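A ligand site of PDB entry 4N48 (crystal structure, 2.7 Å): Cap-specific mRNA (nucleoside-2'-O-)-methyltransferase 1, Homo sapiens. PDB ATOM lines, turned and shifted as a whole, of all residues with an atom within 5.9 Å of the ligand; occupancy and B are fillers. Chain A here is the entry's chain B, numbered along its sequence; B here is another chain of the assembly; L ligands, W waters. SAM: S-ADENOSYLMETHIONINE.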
ATOM      1  N   LEU A 111       2.619  -7.485  14.247  1.00  0.00           N
ATOM      2  CA  LEU A 111       3.311  -7.061  13.021  1.00  0.00           C
ATOM      3  C   LEU A 111       2.624  -7.550  11.739  1.00  0.00           C
ATOM      4  O   LEU A 111       2.750  -6.934  10.684  1.00  0.00           O
ATOM      5  CB  LEU A 111       4.792  -7.429  13.048  1.00  0.00           C
ATOM      6  CG  LEU A 111       5.273  -8.855  13.280  1.00  0.00           C
ATOM      7  CD1 LEU A 111       5.116  -9.724  12.046  1.00  0.00           C
ATOM      8  CD2 LEU A 111       6.723  -8.847  13.739  1.00  0.00           C
ATOM      9  N   ASN A 112       1.917  -8.676  11.841  1.00  0.00           N
ATOM     10  CA  ASN A 112       1.128  -9.159  10.716  1.00  0.00           C
ATOM     11  C   ASN A 112      -0.124  -9.888  11.181  1.00  0.00           C
ATOM     12  O   ASN A 112      -0.395  -9.951  12.378  1.00  0.00           O
ATOM     13  CB  ASN A 112       1.972 -10.014   9.768  1.00  0.00           C
ATOM     14  CG  ASN A 112       2.570 -11.249  10.444  1.00  0.00           C
ATOM     15  OD1 ASN A 112       2.143 -11.650  11.528  1.00  0.00           O
ATOM     16  ND2 ASN A 112       3.561 -11.845   9.798  1.00  0.00           N
ATOM     17  N   ALA A 114      -0.611 -13.034  10.704  1.00  0.00           N
ATOM     18  CA  ALA A 114      -0.186 -14.376  11.074  1.00  0.00           C
ATOM     19  C   ALA A 114      -0.134 -14.546  12.589  1.00  0.00           C
ATOM     20  O   ALA A 114      -0.455 -15.606  13.120  1.00  0.00           O
ATOM     21  CB  ALA A 114       1.161 -14.707  10.453  1.00  0.00           C
ATOM     22  N   ALA A 115       0.250 -13.473  13.291  1.00  0.00           N
ATOM     23  CA  ALA A 115       0.306 -13.503  14.756  1.00  0.00           C
ATOM     24  C   ALA A 115      -1.065 -13.777  15.351  1.00  0.00           C
ATOM     25  O   ALA A 115      -1.192 -14.474  16.356  1.00  0.00           O
ATOM     26  CB  ALA A 115       0.863 -12.198  15.279  1.00  0.00           C
ATOM     27  N   ASP A 153      10.510 -21.624  16.525  1.00  0.00           N
ATOM     28  CA  ASP A 153       9.672 -21.054  15.478  1.00  0.00           C
ATOM     29  C   ASP A 153      10.398 -21.110  14.144  1.00  0.00           C
ATOM     30  O   ASP A 153      11.292 -20.301  13.877  1.00  0.00           O
ATOM     31  CB  ASP A 153       9.300 -19.612  15.825  1.00  0.00           C
ATOM     32  CG  ASP A 153       8.205 -19.055  14.929  1.00  0.00           C
ATOM     33  OD1 ASP A 153       7.532 -19.858  14.240  1.00  0.00           O
ATOM     34  OD2 ASP A 153       8.015 -17.815  14.900  1.00  0.00           O
ATOM     35  N   VAL A 154      10.026 -22.069  13.305  1.00  0.00           N
ATOM     36  CA  VAL A 154      10.703 -22.251  12.023  1.00  0.00           C
ATOM     37  C   VAL A 154       9.854 -21.829  10.821  1.00  0.00           C
ATOM     38  O   VAL A 154       8.620 -21.899  10.867  1.00  0.00           O
ATOM     39  CB  VAL A 154      11.241 -23.691  11.846  1.00  0.00           C
ATOM     40  CG1 VAL A 154      12.169 -24.046  12.994  1.00  0.00           C
ATOM     41  CG2 VAL A 154      10.104 -24.683  11.728  1.00  0.00           C
ATOM     42  N   CYS A 155      10.535 -21.402   9.760  1.00  0.00           N
ATOM     43  CA  CYS A 155       9.902 -20.881   8.556  1.00  0.00           C
ATOM     44  C   CYS A 155       8.944 -19.765   8.940  1.00  0.00           C
ATOM     45  O   CYS A 155       7.736 -19.862   8.714  1.00  0.00           O
ATOM     46  CB  CYS A 155       9.159 -21.991   7.826  1.00  0.00           C
ATOM     47  SG  CYS A 155      10.204 -23.336   7.233  1.00  0.00           S
ATOM     48  N   ALA A 156       9.501 -18.703   9.513  1.00  0.00           N
ATOM     49  CA  ALA A 156       8.724 -17.831  10.388  1.00  0.00           C
ATOM     50  C   ALA A 156       8.872 -16.309  10.242  1.00  0.00           C
ATOM     51  O   ALA A 156       8.245 -15.553  10.986  1.00  0.00           O
ATOM     52  CB  ALA A 156       8.981 -18.232  11.830  1.00  0.00           C
ATOM     53  N   GLY A 157       9.699 -15.842   9.308  1.00  0.00           N
ATOM     54  CA  GLY A 157       9.834 -14.410   9.082  1.00  0.00           C
ATOM     55  C   GLY A 157       8.505 -13.804   8.674  1.00  0.00           C
ATOM     56  O   GLY A 157       7.775 -14.402   7.880  1.00  0.00           O
ATOM     57  N   PRO A 158       8.172 -12.605   9.199  1.00  0.00           N
ATOM     58  CA  PRO A 158       8.942 -11.704  10.066  1.00  0.00           C
ATOM     59  C   PRO A 158       8.923 -12.050  11.563  1.00  0.00           C
ATOM     60  O   PRO A 158       9.736 -11.485  12.311  1.00  0.00           O
ATOM     61  CB  PRO A 158       8.263 -10.335   9.856  1.00  0.00           C
ATOM     62  CG  PRO A 158       7.345 -10.519   8.676  1.00  0.00           C
ATOM     63  CD  PRO A 158       6.938 -11.953   8.713  1.00  0.00           C
ATOM     64  N   GLY A 159       8.027 -12.933  12.007  1.00  0.00           N
ATOM     65  CA  GLY A 159       8.052 -13.434  13.375  1.00  0.00           C
ATOM     66  C   GLY A 159       6.783 -13.265  14.195  1.00  0.00           C
ATOM     67  O   GLY A 159       6.835 -13.312  15.424  1.00  0.00           O
ATOM     68  N   GLY A 160       5.653 -13.095  13.513  1.00  0.00           N
ATOM     69  CA  GLY A 160       4.365 -12.898  14.177  1.00  0.00           C
ATOM     70  C   GLY A 160       3.978 -13.980  15.168  1.00  0.00           C
ATOM     71  O   GLY A 160       3.425 -13.670  16.224  1.00  0.00           O
ATOM     72  N   PHE A 161       4.270 -15.239  14.846  1.00  0.00           N
ATOM     73  CA  PHE A 161       3.969 -16.353  15.749  1.00  0.00           C
ATOM     74  C   PHE A 161       4.709 -16.207  17.061  1.00  0.00           C
ATOM     75  O   PHE A 161       4.154 -16.413  18.140  1.00  0.00           O
ATOM     76  CB  PHE A 161       4.329 -17.701  15.113  1.00  0.00           C
ATOM     77  CG  PHE A 161       3.287 -18.239  14.172  1.00  0.00           C
ATOM     78  CD1 PHE A 161       2.297 -17.407  13.653  1.00  0.00           C
ATOM     79  CD2 PHE A 161       3.281 -19.568  13.804  1.00  0.00           C
ATOM     80  CE1 PHE A 161       1.341 -17.901  12.779  1.00  0.00           C
ATOM     81  CE2 PHE A 161       2.317 -20.066  12.941  1.00  0.00           C
ATOM     82  CZ  PHE A 161       1.355 -19.234  12.424  1.00  0.00           C
ATOM     83  N   SER A 162       5.992 -15.852  16.978  1.00  0.00           N
ATOM     84  CA  SER A 162       6.803 -15.646  18.163  1.00  0.00           C
ATOM     85  C   SER A 162       6.404 -14.368  18.890  1.00  0.00           C
ATOM     86  O   SER A 162       6.494 -14.296  20.118  1.00  0.00           O
ATOM     87  CB  SER A 162       8.288 -15.594  17.788  1.00  0.00           C
ATOM     88  OG  SER A 162       8.731 -16.856  17.342  1.00  0.00           O
ATOM     89  N   MET A 178      14.386 -20.128  13.147  1.00  0.00           N
ATOM     90  CA  MET A 178      15.087 -20.205  11.869  1.00  0.00           C
ATOM     91  C   MET A 178      14.133 -19.911  10.715  1.00  0.00           C
ATOM     92  O   MET A 178      13.006 -20.414  10.686  1.00  0.00           O
ATOM     93  CB  MET A 178      15.771 -21.562  11.689  1.00  0.00           C
ATOM     94  CG  MET A 178      16.501 -21.712  10.340  1.00  0.00           C
ATOM     95  SD  MET A 178      17.419 -23.255  10.161  1.00  0.00           S
ATOM     96  CE  MET A 178      16.147 -24.454  10.582  1.00  0.00           C
ATOM     97  N   THR A 179      14.590 -19.084   9.782  1.00  0.00           N
ATOM     98  CA  THR A 179      13.821 -18.736   8.597  1.00  0.00           C
ATOM     99  C   THR A 179      14.767 -18.298   7.481  1.00  0.00           C
ATOM    100  O   THR A 179      15.930 -17.997   7.728  1.00  0.00           O
ATOM    101  CB  THR A 179      12.799 -17.621   8.881  1.00  0.00           C
ATOM    102  OG1 THR A 179      11.841 -17.543   7.821  1.00  0.00           O
ATOM    103  CG2 THR A 179      13.502 -16.282   9.031  1.00  0.00           C
ATOM    104  N   LEU A 180      14.269 -18.253   6.248  1.00  0.00           N
ATOM    105  CA  LEU A 180      15.066 -17.787   5.113  1.00  0.00           C
ATOM    106  C   LEU A 180      15.468 -16.318   5.222  1.00  0.00           C
ATOM    107  O   LEU A 180      14.622 -15.445   5.371  1.00  0.00           O
ATOM    108  CB  LEU A 180      14.313 -17.990   3.806  1.00  0.00           C
ATOM    109  CG  LEU A 180      14.450 -19.343   3.122  1.00  0.00           C
ATOM    110  CD1 LEU A 180      13.754 -19.300   1.769  1.00  0.00           C
ATOM    111  CD2 LEU A 180      15.908 -19.725   2.974  1.00  0.00           C
ATOM    112  N   ASN A 184      12.121 -11.397   3.708  1.00  0.00           N
ATOM    113  CA  ASN A 184      11.173 -12.002   4.631  1.00  0.00           C
ATOM    114  C   ASN A 184      11.855 -12.563   5.871  1.00  0.00           C
ATOM    115  O   ASN A 184      11.378 -13.529   6.457  1.00  0.00           O
ATOM    116  CB  ASN A 184      10.363 -13.095   3.942  1.00  0.00           C
ATOM    117  CG  ASN A 184       9.437 -12.557   2.866  1.00  0.00           C
ATOM    118  OD1 ASN A 184       8.895 -11.448   2.993  1.00  0.00           O
ATOM    119  ND2 ASN A 184       9.243 -13.327   1.800  1.00  0.00           N
ATOM    120  N   ASP A 185      12.967 -11.945   6.252  1.00  0.00           N
ATOM    121  CA  ASP A 185      13.712 -12.369   7.426  1.00  0.00           C
ATOM    122  C   ASP A 185      12.996 -11.911   8.698  1.00  0.00           C
ATOM    123  O   ASP A 185      12.013 -11.175   8.636  1.00  0.00           O
ATOM    124  CB  ASP A 185      15.131 -11.786   7.383  1.00  0.00           C
ATOM    125  CG  ASP A 185      16.120 -12.579   8.213  1.00  0.00           C
ATOM    126  OD1 ASP A 185      15.689 -13.378   9.067  1.00  0.00           O
ATOM    127  OD2 ASP A 185      17.347 -12.393   8.008  1.00  0.00           O
ATOM    128  N   GLY A 212      19.509 -20.052   6.595  1.00  0.00           N
ATOM    129  CA  GLY A 212      18.259 -20.407   7.234  1.00  0.00           C
ATOM    130  C   GLY A 212      17.374 -21.328   6.405  1.00  0.00           C
ATOM    131  O   GLY A 212      16.217 -21.552   6.753  1.00  0.00           O
ATOM    132  N   ASP A 213      17.917 -21.861   5.319  1.00  0.00           N
ATOM    133  CA  ASP A 213      17.175 -22.806   4.499  1.00  0.00           C
ATOM    134  C   ASP A 213      16.995 -24.108   5.278  1.00  0.00           C
ATOM    135  O   ASP A 213      17.949 -24.830   5.543  1.00  0.00           O
ATOM    136  CB  ASP A 213      17.873 -23.064   3.158  1.00  0.00           C
ATOM    137  CG  ASP A 213      16.985 -23.765   2.151  1.00  0.00           C
ATOM    138  OD1 ASP A 213      15.914 -24.275   2.546  1.00  0.00           O
ATOM    139  OD2 ASP A 213      17.345 -23.802   0.958  1.00  0.00           O
ATOM    140  N   ILE A 214      15.746 -24.391   5.656  1.00  0.00           N
ATOM    141  CA  ILE A 214      15.409 -25.542   6.484  1.00  0.00           C
ATOM    142  C   ILE A 214      15.474 -26.837   5.673  1.00  0.00           C
ATOM    143  O   ILE A 214      15.401 -27.934   6.235  1.00  0.00           O
ATOM    144  CB  ILE A 214      13.990 -25.368   7.102  1.00  0.00           C
ATOM    145  CG1 ILE A 214      13.784 -26.319   8.279  1.00  0.00           C
ATOM    146  CG2 ILE A 214      12.915 -25.546   6.033  1.00  0.00           C
ATOM    147  CD1 ILE A 214      12.444 -26.134   8.984  1.00  0.00           C
ATOM    148  N   THR A 215      15.610 -26.723   4.356  1.00  0.00           N
ATOM    149  CA  THR A 215      15.659 -27.899   3.500  1.00  0.00           C
ATOM    150  C   THR A 215      17.076 -28.408   3.301  1.00  0.00           C
ATOM    151  O   THR A 215      17.294 -29.358   2.549  1.00  0.00           O
ATOM    152  CB  THR A 215      15.006 -27.647   2.132  1.00  0.00           C
ATOM    153  OG1 THR A 215      15.713 -26.599   1.458  1.00  0.00           O
ATOM    154  CG2 THR A 215      13.552 -27.236   2.303  1.00  0.00           C
ATOM    155  N   ASP A 242       5.330 -22.399  10.005  1.00  0.00           N
ATOM    156  CA  ASP A 242       4.326 -21.751   9.163  1.00  0.00           C
ATOM    157  C   ASP A 242       4.879 -21.440   7.760  1.00  0.00           C
ATOM    158  O   ASP A 242       4.605 -20.371   7.199  1.00  0.00           O
ATOM    159  CB  ASP A 242       3.845 -20.473   9.841  1.00  0.00           C
ATOM    160  CG  ASP A 242       2.560 -19.934   9.247  1.00  0.00           C
ATOM    161  OD1 ASP A 242       1.665 -20.743   8.908  1.00  0.00           O
ATOM    162  OD2 ASP A 242       2.448 -18.706   9.123  1.00  0.00           O
ATOM    163  N   GLY A 243       5.629 -22.391   7.198  1.00  0.00           N
ATOM    164  CA  GLY A 243       6.319 -22.186   5.931  1.00  0.00           C
ATOM    165  C   GLY A 243       5.470 -22.032   4.669  1.00  0.00           C
ATOM    166  O   GLY A 243       4.491 -22.742   4.472  1.00  0.00           O
ATOM    167  N   GLY A 244       5.890 -21.110   3.810  1.00  0.00           N
ATOM    168  CA  GLY A 244       5.222 -20.850   2.543  1.00  0.00           C
ATOM    169  C   GLY A 244       6.049 -19.938   1.647  1.00  0.00           C
ATOM    170  O   GLY A 244       7.000 -19.290   2.089  1.00  0.00           O
ATOM    171  N   PHE A 245       5.696 -19.905   0.366  1.00  0.00           N
ATOM    172  CA  PHE A 245       6.358 -19.013  -0.590  1.00  0.00           C
ATOM    173  C   PHE A 245       5.446 -18.809  -1.777  1.00  0.00           C
ATOM    174  O   PHE A 245       4.408 -19.446  -1.895  1.00  0.00           O
ATOM    175  CB  PHE A 245       7.715 -19.581  -1.016  1.00  0.00           C
ATOM    176  CG  PHE A 245       7.664 -20.993  -1.510  1.00  0.00           C
ATOM    177  CD1 PHE A 245       7.203 -21.292  -2.786  1.00  0.00           C
ATOM    178  CD2 PHE A 245       8.097 -22.038  -0.703  1.00  0.00           C
ATOM    179  CE1 PHE A 245       7.167 -22.597  -3.247  1.00  0.00           C
ATOM    180  CE2 PHE A 245       8.066 -23.348  -1.152  1.00  0.00           C
ATOM    181  CZ  PHE A 245       7.598 -23.624  -2.425  1.00  0.00           C
ATOM    182  N   LEU A 261       9.284 -28.679   1.760  1.00  0.00           N
ATOM    183  CA  LEU A 261       9.177 -27.747   2.871  1.00  0.00           C
ATOM    184  C   LEU A 261       8.339 -28.377   3.978  1.00  0.00           C
ATOM    185  O   LEU A 261       8.656 -28.253   5.168  1.00  0.00           O
ATOM    186  CB  LEU A 261       8.492 -26.467   2.404  1.00  0.00           C
ATOM    187  CG  LEU A 261       8.955 -25.102   2.914  1.00  0.00           C
ATOM    188  CD1 LEU A 261       7.756 -24.217   3.230  1.00  0.00           C
ATOM    189  CD2 LEU A 261       9.893 -25.204   4.094  1.00  0.00           C
ATOM    190  N   LYS A 282       1.717 -25.393   9.504  1.00  0.00           N
ATOM    191  CA  LYS A 282       0.858 -25.030   8.380  1.00  0.00           C
ATOM    192  C   LYS A 282       1.060 -25.992   7.234  1.00  0.00           C
ATOM    193  O   LYS A 282       2.198 -26.292   6.858  1.00  0.00           O
ATOM    194  CB  LYS A 282       1.154 -23.612   7.890  1.00  0.00           C
ATOM    195  CG  LYS A 282       0.066 -23.023   6.974  1.00  0.00           C
ATOM    196  CD  LYS A 282       0.585 -22.619   5.594  1.00  0.00           C
ATOM    197  CE  LYS A 282       1.584 -21.459   5.663  1.00  0.00           C
ATOM    198  NZ  LYS A 282       1.017 -20.225   6.273  1.00  0.00           N
ATOM    199  O5'   G B   1      -1.374 -17.882   1.322  1.00  0.00           O
ATOM    200  C5'   G B   1      -1.560 -18.461   2.612  1.00  0.00           C
ATOM    201  C4'   G B   1      -0.309 -18.363   3.446  1.00  0.00           C
ATOM    202  O4'   G B   1       0.807 -18.931   2.709  1.00  0.00           O
ATOM    203  C3'   G B   1       0.143 -16.963   3.799  1.00  0.00           C
ATOM    204  O3'   G B   1      -0.517 -16.447   4.933  1.00  0.00           O
ATOM    205  C2'   G B   1       1.646 -17.132   4.000  1.00  0.00           C
ATOM    206  O2'   G B   1       1.915 -17.707   5.273  1.00  0.00           O
ATOM    207  C1'   G B   1       1.968 -18.167   2.926  1.00  0.00           C
ATOM    208  N9    G B   1       2.321 -17.524   1.641  1.00  0.00           N
ATOM    209  C8    G B   1       1.566 -17.593   0.493  1.00  0.00           C
ATOM    210  N7    G B   1       2.077 -16.932  -0.512  1.00  0.00           N
ATOM    211  C5    G B   1       3.240 -16.390   0.009  1.00  0.00           C
ATOM    212  C6    G B   1       4.207 -15.557  -0.613  1.00  0.00           C
ATOM    213  O6    G B   1       4.222 -15.153  -1.783  1.00  0.00           O
ATOM    214  N1    G B   1       5.225 -15.221   0.270  1.00  0.00           N
ATOM    215  C2    G B   1       5.307 -15.619   1.581  1.00  0.00           C
ATOM    216  N2    G B   1       6.363 -15.191   2.273  1.00  0.00           N
ATOM    217  N3    G B   1       4.403 -16.394   2.171  1.00  0.00           N
ATOM    218  C4    G B   1       3.404 -16.738   1.334  1.00  0.00           C
ATOM    219  P     A B   2      -1.108 -14.952   4.923  1.00  0.00           P
ATOM    220  OP1   A B   2      -2.030 -14.838   6.089  1.00  0.00           O
ATOM    221  OP2   A B   2      -1.623 -14.634   3.568  1.00  0.00           O
ATOM    222  O5'   A B   2       0.163 -14.041   5.211  1.00  0.00           O
ATOM    223  C5'   A B   2       0.791 -14.021   6.477  1.00  0.00           C
ATOM    224  C4'   A B   2       1.997 -13.122   6.471  1.00  0.00           C
ATOM    225  O4'   A B   2       3.009 -13.674   5.595  1.00  0.00           O
ATOM    226  C3'   A B   2       1.779 -11.719   5.944  1.00  0.00           C
ATOM    227  O3'   A B   2       1.204 -10.845   6.887  1.00  0.00           O
ATOM    228  C2'   A B   2       3.176 -11.309   5.510  1.00  0.00           C
ATOM    229  O2'   A B   2       3.987 -11.003   6.635  1.00  0.00           O
ATOM    230  C1'   A B   2       3.680 -12.620   4.916  1.00  0.00           C
ATOM    231  N9    A B   2       3.350 -12.711   3.486  1.00  0.00           N
ATOM    232  C8    A B   2       2.302 -13.390   2.919  1.00  0.00           C
ATOM    233  N7    A B   2       2.239 -13.276   1.618  1.00  0.00           N
ATOM    234  C5    A B   2       3.305 -12.446   1.307  1.00  0.00           C
ATOM    235  C6    A B   2       3.767 -11.953   0.085  1.00  0.00           C
ATOM    236  N6    A B   2       3.192 -12.233  -1.092  1.00  0.00           N
ATOM    237  N1    A B   2       4.855 -11.147   0.096  1.00  0.00           N
ATOM    238  C2    A B   2       5.436 -10.871   1.285  1.00  0.00           C
ATOM    239  N3    A B   2       5.084 -11.290   2.505  1.00  0.00           N
ATOM    240  C4    A B   2       3.999 -12.079   2.447  1.00  0.00           C
HETATM  241  N   SAM L   1       4.689 -17.419  10.863  1.00  0.00           N
HETATM  242  CA  SAM L   1       5.218 -16.220  10.215  1.00  0.00           C
HETATM  243  C   SAM L   1       4.888 -15.009  11.008  1.00  0.00           C
HETATM  244  O   SAM L   1       4.024 -15.097  11.955  1.00  0.00           O
HETATM  245  OXT SAM L   1       5.436 -13.940  10.774  1.00  0.00           O
HETATM  246  CB  SAM L   1       4.639 -16.082   8.855  1.00  0.00           C
HETATM  247  CG  SAM L   1       4.907 -17.198   7.883  1.00  0.00           C
HETATM  248  SD  SAM L   1       5.795 -16.760   6.367  1.00  0.00           S
HETATM  249  CE  SAM L   1       4.668 -16.088   5.257  1.00  0.00           C
HETATM  250  C5' SAM L   1       6.527 -18.183   5.626  1.00  0.00           C
HETATM  251  C4' SAM L   1       8.026 -18.213   5.724  1.00  0.00           C
HETATM  252  O4' SAM L   1       8.530 -19.471   5.314  1.00  0.00           O
HETATM  253  C3' SAM L   1       8.628 -17.229   4.861  1.00  0.00           C
HETATM  254  O3' SAM L   1       9.237 -16.247   5.639  1.00  0.00           O
HETATM  255  C2' SAM L   1       9.626 -17.987   4.085  1.00  0.00           C
HETATM  256  O2' SAM L   1      10.794 -17.268   3.920  1.00  0.00           O
HETATM  257  C1' SAM L   1       9.837 -19.153   4.899  1.00  0.00           C
HETATM  258  N9  SAM L   1      10.403 -20.160   4.160  1.00  0.00           N
HETATM  259  C8  SAM L   1       9.995 -20.637   2.950  1.00  0.00           C
HETATM  260  N7  SAM L   1      10.833 -21.608   2.567  1.00  0.00           N
HETATM  261  C5  SAM L   1      11.789 -21.764   3.513  1.00  0.00           C
HETATM  262  C6  SAM L   1      12.911 -22.602   3.669  1.00  0.00           C
HETATM  263  N6  SAM L   1      13.249 -23.588   2.634  1.00  0.00           N
HETATM  264  N1  SAM L   1      13.661 -22.484   4.760  1.00  0.00           N
HETATM  265  C2  SAM L   1      13.366 -21.569   5.724  1.00  0.00           C
HETATM  266  N3  SAM L   1      12.305 -20.750   5.622  1.00  0.00           N
HETATM  267  C4  SAM L   1      11.503 -20.831   4.536  1.00  0.00           C
HETATM  268  O   HOH W   1      11.365 -15.031   1.544  1.00  0.00           O
HETATM  269  O   HOH W   2      12.210 -16.077   5.944  1.00  0.00           O
HETATM  270  O   HOH W   3       6.078 -19.536  11.900  1.00  0.00           O
HETATM  271  O   HOH W   4       6.619 -16.376  13.233  1.00  0.00           O
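The side-chain carboxylate of Asp 242 lies within salt-bridge range of the side-chain amino group of Lys 282. N of Asp 242 is in hydrogen-bond range of O of Val 154 (3.4 Å). N of Ala 114 sits at hydrogen-bond distance from OD1 of Asn 112 (3.2 Å). O2' of G 1 of chain B is in hydrogen-bond range of the side-chain amino group of Lys 282 (2.9 Å). OG1 of Thr 215 is in hydrogen-bond range of OD1 of Asp 213, at 2.6 Å. O2' of A 2 of chain B lies within hydrogen-bond range of the side-chain amide nitrogen of Asn 112 (3.3 Å). OG1 of Thr 179 sits at hydrogen-bond distance from N of Ala 156 (3.1 Å). The backbone NH of Gly 157 lies within hydrogen-bond range of the side-chain hydroxyl of Thr 179 (3.1 Å).
Water W3 lies within hydrogen-bond range of N of the ligand and OD1 of Asp 153. Water W2 lies within hydrogen-bond range of the side-chain hydroxyl of Thr 179, the backbone carbonyl oxygen of Leu 180, the backbone carbonyl oxygen of Asn 184 and an oxygen (O2') of the ligand. Water W4 lies within hydrogen-bond range of the side-chain carboxylate of Asp 153 (2.6 Å), the backbone carbonyl oxygen of Ala 156 (2.9 Å), the backbone NH of Phe 161 (3.1 Å), an oxygen (O) of the ligand (3.2 Å) and the backbone NH of Gly 160 (3.4 Å). Water W1 bridges ND2 of Asn 184 (2.7 Å) and O2' of the ligand (3.3 Å).
The side-chain carboxylate of Asp 242 lies within salt-bridge range of a nitrogen (N) of the ligand (3.1 Å). ND2 of Asn 112 lies within hydrogen-bond range of OXT of the ligand (3.0 Å). The backbone NH of Gly 159 lies within hydrogen-bond range of an oxygen (OXT) of the ligand (3.0 Å). The backbone NH (N) of Gly 160 lies within hydrogen-bond range of an oxygen (OXT) of the ligand. The backbone NH (N) of Gly 244 lies within hydrogen-bond range of an oxygen (O4') of the ligand (3.5 Å). A nitrogen (N3) of the ligand sits at hydrogen-bond distance from the side-chain sulfur of Cys 155. An oxygen (O3') of the ligand is in hydrogen-bond range of the backbone carbonyl oxygen of Gly 157, at 3.3 Å. The backbone NH (N) of Ile 214 is in hydrogen-bond range of a nitrogen (N1) of the ligand, 3.0 Å away. The side-chain carboxylate of Asp 213 lies within hydrogen-bond range of a nitrogen (N6) of the ligand (2.8 Å). N of Phe 161 is in hydrogen-bond range of O of the ligand (2.9 Å). N of Leu 180 sits at hydrogen-bond distance from N3 of the ligand (3.2 Å).
The backbone carbonyl oxygen (O) of Ala 156 lies close to an oxygen (OXT) of the ligand, 3.2 Å away. N of Pro 158 sits close to OXT of the ligand, 3.4 Å away. The backbone carbonyl oxygen of Gly 212 lies close to a nitrogen (N1) of the ligand. Merely in contact with the ligand: Ala 114 (3.3 Å), Thr 179 (3.6 Å), Asn 184 (3.6 Å), Thr 215 (3.7 Å), Gly 243 (3.6 Å), Leu 261 (3.97 Å), G 1 of chain B (3.1 Å) and A 2 of chain B (2.9 Å). Within 4 Å of the ligand: Asn 112, Ala 114, Cys 155, Ala 156, Gly 157, Pro 158, Gly 159, Gly 160, Phe 161, Thr 179, Leu 180, Asn 184, Gly 212, Asp 213, Ile 214, Thr 215, Asp 242, Gly 243, Gly 244, Leu 261, G 1 of chain B and A 2 of chain B. Along chain A the residues within 4 Å of the ligand span positions 112 to 261.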
